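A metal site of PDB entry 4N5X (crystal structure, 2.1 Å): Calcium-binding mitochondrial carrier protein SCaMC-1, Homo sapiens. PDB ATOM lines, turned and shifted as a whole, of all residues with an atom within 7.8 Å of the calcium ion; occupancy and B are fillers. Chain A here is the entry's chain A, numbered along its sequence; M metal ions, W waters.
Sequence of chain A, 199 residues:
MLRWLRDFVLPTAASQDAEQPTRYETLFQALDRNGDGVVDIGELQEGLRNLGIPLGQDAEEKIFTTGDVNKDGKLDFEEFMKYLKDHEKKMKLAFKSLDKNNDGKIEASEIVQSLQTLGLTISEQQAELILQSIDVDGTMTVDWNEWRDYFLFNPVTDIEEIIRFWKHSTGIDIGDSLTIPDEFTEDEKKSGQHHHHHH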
ATOM      1  N   PHE A  28     -10.358  -0.455 -15.787  1.00  0.00           N
ATOM      2  CA  PHE A  28     -10.981  -1.342 -14.808  1.00  0.00           C
ATOM      3  C   PHE A  28      -9.937  -2.212 -14.111  1.00  0.00           C
ATOM      4  O   PHE A  28      -9.897  -2.266 -12.875  1.00  0.00           O
ATOM      5  CB  PHE A  28     -12.049  -2.210 -15.461  1.00  0.00           C
ATOM      6  CG  PHE A  28     -12.880  -2.994 -14.473  1.00  0.00           C
ATOM      7  CD1 PHE A  28     -13.914  -2.375 -13.772  1.00  0.00           C
ATOM      8  CD2 PHE A  28     -12.629  -4.340 -14.245  1.00  0.00           C
ATOM      9  CE1 PHE A  28     -14.679  -3.098 -12.857  1.00  0.00           C
ATOM     10  CE2 PHE A  28     -13.394  -5.063 -13.330  1.00  0.00           C
ATOM     11  CZ  PHE A  28     -14.421  -4.447 -12.635  1.00  0.00           C
ATOM     12  N   LEU A  31      -7.739  -0.426 -11.719  1.00  0.00           N
ATOM     13  CA  LEU A  31      -8.480  -0.139 -10.497  1.00  0.00           C
ATOM     14  C   LEU A  31      -8.646  -1.377  -9.617  1.00  0.00           C
ATOM     15  O   LEU A  31      -8.534  -1.296  -8.390  1.00  0.00           O
ATOM     16  CB  LEU A  31      -9.870   0.405 -10.853  1.00  0.00           C
ATOM     17  CG  LEU A  31     -10.161   1.912 -10.791  1.00  0.00           C
ATOM     18  CD1 LEU A  31      -8.936   2.766 -10.458  1.00  0.00           C
ATOM     19  CD2 LEU A  31     -10.825   2.390 -12.069  1.00  0.00           C
ATOM     20  N   ASP A  32      -8.924  -2.520 -10.233  1.00  0.00           N
ATOM     21  CA  ASP A  32      -9.140  -3.752  -9.467  1.00  0.00           C
ATOM     22  C   ASP A  32      -7.827  -4.286  -8.908  1.00  0.00           C
ATOM     23  O   ASP A  32      -7.303  -5.284  -9.384  1.00  0.00           O
ATOM     24  CB  ASP A  32      -9.835  -4.803 -10.332  1.00  0.00           C
ATOM     25  CG  ASP A  32     -10.064  -6.109  -9.588  1.00  0.00           C
ATOM     26  OD1 ASP A  32      -9.939  -6.127  -8.353  1.00  0.00           O
ATOM     27  OD2 ASP A  32     -10.385  -7.118 -10.248  1.00  0.00           O
ATOM     28  N   ARG A  33      -7.328  -3.630  -7.866  1.00  0.00           N
ATOM     29  CA  ARG A  33      -6.005  -3.946  -7.323  1.00  0.00           C
ATOM     30  C   ARG A  33      -5.848  -5.361  -6.769  1.00  0.00           C
ATOM     31  O   ARG A  33      -4.828  -5.996  -6.997  1.00  0.00           O
ATOM     32  CB  ARG A  33      -5.577  -2.914  -6.283  1.00  0.00           C
ATOM     33  CG  ARG A  33      -4.266  -2.214  -6.636  1.00  0.00           C
ATOM     34  CD  ARG A  33      -3.751  -1.343  -5.500  1.00  0.00           C
ATOM     35  NE  ARG A  33      -2.297  -1.307  -5.483  1.00  0.00           N
ATOM     36  CZ  ARG A  33      -1.567  -0.435  -6.177  1.00  0.00           C
ATOM     37  NH1 ARG A  33      -2.150   0.472  -6.944  1.00  0.00           N
ATOM     38  NH2 ARG A  33      -0.237  -0.485  -6.092  1.00  0.00           N
ATOM     39  N   ASN A  34      -6.844  -5.851  -6.047  1.00  0.00           N
ATOM     40  CA  ASN A  34      -6.766  -7.207  -5.489  1.00  0.00           C
ATOM     41  C   ASN A  34      -7.177  -8.312  -6.483  1.00  0.00           C
ATOM     42  O   ASN A  34      -7.241  -9.488  -6.131  1.00  0.00           O
ATOM     43  CB  ASN A  34      -7.567  -7.324  -4.187  1.00  0.00           C
ATOM     44  CG  ASN A  34      -9.081  -7.268  -4.394  1.00  0.00           C
ATOM     45  OD1 ASN A  34      -9.574  -7.216  -5.523  1.00  0.00           O
ATOM     46  ND2 ASN A  34      -9.820  -7.272  -3.300  1.00  0.00           N
ATOM     47  N   GLY A  35      -7.494  -7.897  -7.711  1.00  0.00           N
ATOM     48  CA  GLY A  35      -7.879  -8.799  -8.774  1.00  0.00           C
ATOM     49  C   GLY A  35      -9.053  -9.720  -8.512  1.00  0.00           C
ATOM     50  O   GLY A  35      -9.073 -10.836  -9.036  1.00  0.00           O
ATOM     51  N   ASP A  36     -10.031  -9.294  -7.717  1.00  0.00           N
ATOM     52  CA  ASP A  36     -11.208 -10.128  -7.508  1.00  0.00           C
ATOM     53  C   ASP A  36     -12.279  -9.938  -8.574  1.00  0.00           C
ATOM     54  O   ASP A  36     -13.378 -10.483  -8.456  1.00  0.00           O
ATOM     55  CB  ASP A  36     -11.796  -9.965  -6.098  1.00  0.00           C
ATOM     56  CG  ASP A  36     -12.280  -8.555  -5.812  1.00  0.00           C
ATOM     57  OD1 ASP A  36     -12.337  -7.723  -6.739  1.00  0.00           O
ATOM     58  OD2 ASP A  36     -12.620  -8.271  -4.642  1.00  0.00           O
ATOM     59  N   GLY A  37     -11.966  -9.162  -9.609  1.00  0.00           N
ATOM     60  CA  GLY A  37     -12.882  -8.999 -10.724  1.00  0.00           C
ATOM     61  C   GLY A  37     -13.888  -7.873 -10.595  1.00  0.00           C
ATOM     62  O   GLY A  37     -14.652  -7.599 -11.527  1.00  0.00           O
ATOM     63  N   VAL A  38     -13.917  -7.213  -9.437  1.00  0.00           N
ATOM     64  CA  VAL A  38     -14.804  -6.063  -9.248  1.00  0.00           C
ATOM     65  C   VAL A  38     -14.039  -4.908  -8.624  1.00  0.00           C
ATOM     66  O   VAL A  38     -12.937  -5.079  -8.095  1.00  0.00           O
ATOM     67  CB  VAL A  38     -16.021  -6.394  -8.350  1.00  0.00           C
ATOM     68  CG1 VAL A  38     -16.875  -7.441  -9.009  1.00  0.00           C
ATOM     69  CG2 VAL A  38     -15.566  -6.860  -6.980  1.00  0.00           C
ATOM     70  N   VAL A  39     -14.626  -3.725  -8.710  1.00  0.00           N
ATOM     71  CA  VAL A  39     -13.993  -2.554  -8.120  1.00  0.00           C
ATOM     72  C   VAL A  39     -14.767  -2.125  -6.885  1.00  0.00           C
ATOM     73  O   VAL A  39     -15.966  -1.840  -6.966  1.00  0.00           O
ATOM     74  CB  VAL A  39     -13.894  -1.393  -9.132  1.00  0.00           C
ATOM     75  CG1 VAL A  39     -13.452  -0.117  -8.432  1.00  0.00           C
ATOM     76  CG2 VAL A  39     -12.934  -1.757 -10.267  1.00  0.00           C
ATOM     77  N   ASP A  40     -14.098  -2.082  -5.735  1.00  0.00           N
ATOM     78  CA  ASP A  40     -14.770  -1.670  -4.519  1.00  0.00           C
ATOM     79  C   ASP A  40     -14.523  -0.180  -4.287  1.00  0.00           C
ATOM     80  O   ASP A  40     -13.712   0.439  -4.990  1.00  0.00           O
ATOM     81  CB  ASP A  40     -14.402  -2.550  -3.294  1.00  0.00           C
ATOM     82  CG  ASP A  40     -12.935  -2.478  -2.936  1.00  0.00           C
ATOM     83  OD1 ASP A  40     -12.398  -1.346  -2.850  1.00  0.00           O
ATOM     84  OD2 ASP A  40     -12.314  -3.540  -2.713  1.00  0.00           O
ATOM     85  N   GLU A  43     -10.940   0.837  -3.649  1.00  0.00           N
ATOM     86  CA  GLU A  43     -10.146   0.768  -4.870  1.00  0.00           C
ATOM     87  C   GLU A  43     -10.410   1.985  -5.766  1.00  0.00           C
ATOM     88  O   GLU A  43      -9.476   2.557  -6.328  1.00  0.00           O
ATOM     89  CB  GLU A  43     -10.458  -0.537  -5.614  1.00  0.00           C
ATOM     90  CG  GLU A  43      -9.875  -1.784  -4.950  1.00  0.00           C
ATOM     91  CD  GLU A  43     -10.260  -3.031  -5.682  1.00  0.00           C
ATOM     92  OE1 GLU A  43     -11.375  -3.045  -6.253  1.00  0.00           O
ATOM     93  OE2 GLU A  43      -9.453  -3.987  -5.714  1.00  0.00           O
ATOM     94  N   LYS A  74     -20.217  -3.266  -4.968  1.00  0.00           N
ATOM     95  CA  LYS A  74     -19.102  -3.377  -5.898  1.00  0.00           C
ATOM     96  C   LYS A  74     -19.541  -2.883  -7.265  1.00  0.00           C
ATOM     97  O   LYS A  74     -20.713  -2.932  -7.601  1.00  0.00           O
ATOM     98  CB  LYS A  74     -18.645  -4.836  -6.038  1.00  0.00           C
ATOM     99  CG  LYS A  74     -18.659  -5.640  -4.731  1.00  0.00           C
ATOM    100  CD  LYS A  74     -18.436  -7.121  -5.005  1.00  0.00           C
ATOM    101  CE  LYS A  74     -19.489  -7.987  -4.334  1.00  0.00           C
ATOM    102  NZ  LYS A  74     -19.705  -7.601  -2.908  1.00  0.00           N
ATOM    103  N   LEU A  75     -18.585  -2.382  -8.056  1.00  0.00           N
ATOM    104  CA  LEU A  75     -18.845  -2.071  -9.454  1.00  0.00           C
ATOM    105  C   LEU A  75     -18.285  -3.201 -10.292  1.00  0.00           C
ATOM    106  O   LEU A  75     -17.083  -3.420 -10.311  1.00  0.00           O
ATOM    107  CB  LEU A  75     -18.143  -0.768  -9.884  1.00  0.00           C
ATOM    108  CG  LEU A  75     -18.644   0.580  -9.384  1.00  0.00           C
ATOM    109  CD1 LEU A  75     -17.775   1.700  -9.990  1.00  0.00           C
ATOM    110  CD2 LEU A  75     -20.115   0.770  -9.717  1.00  0.00           C
HETATM  111 CA    CA M   1     -11.341  -5.594  -6.567  1.00  0.00          CA
HETATM  112  O   HOH W   1     -12.445  -5.713  -4.482  1.00  0.00           O
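OD1 of Asp 32 sits close to N of Gly 35 (3.1 Å).
OD2 of Asp 32 sits at hydrogen-bond distance from N of Gly 37, at 2.7 Å.
The backbone NH (N) of Glu 43 is in hydrogen-bond range of the side-chain carboxylate (OD1) of Asp 40 (2.7 Å).
The backbone NH (N) of Arg 33 lies close to the side-chain carboxylate (OE2) of Glu 43 (3.0 Å).
Of the 14 residues printed, 5 come within 4 Å of the calcium ion.
The nearest printed residue that does not touch the calcium ion is Val 39 (4.3 Å).
The calcium ion is bound by O of Val 38 (2.3 Å), OD1 of Asp 32 (2.3 Å), OD1 of Asp 36 (2.4 Å), water W1 (2.4 Å), OE1 of Glu 43 (2.6 Å), OD1 of Asn 34 (2.6 Å) and OE2 of Glu 43 (2.6 Å).
Water W1 lies within hydrogen-bond range of OD2 of Asp 36 (2.6 Å), OD2 of Asp 40 (2.8 Å) and ND2 of Asn 34 (3.3 Å).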
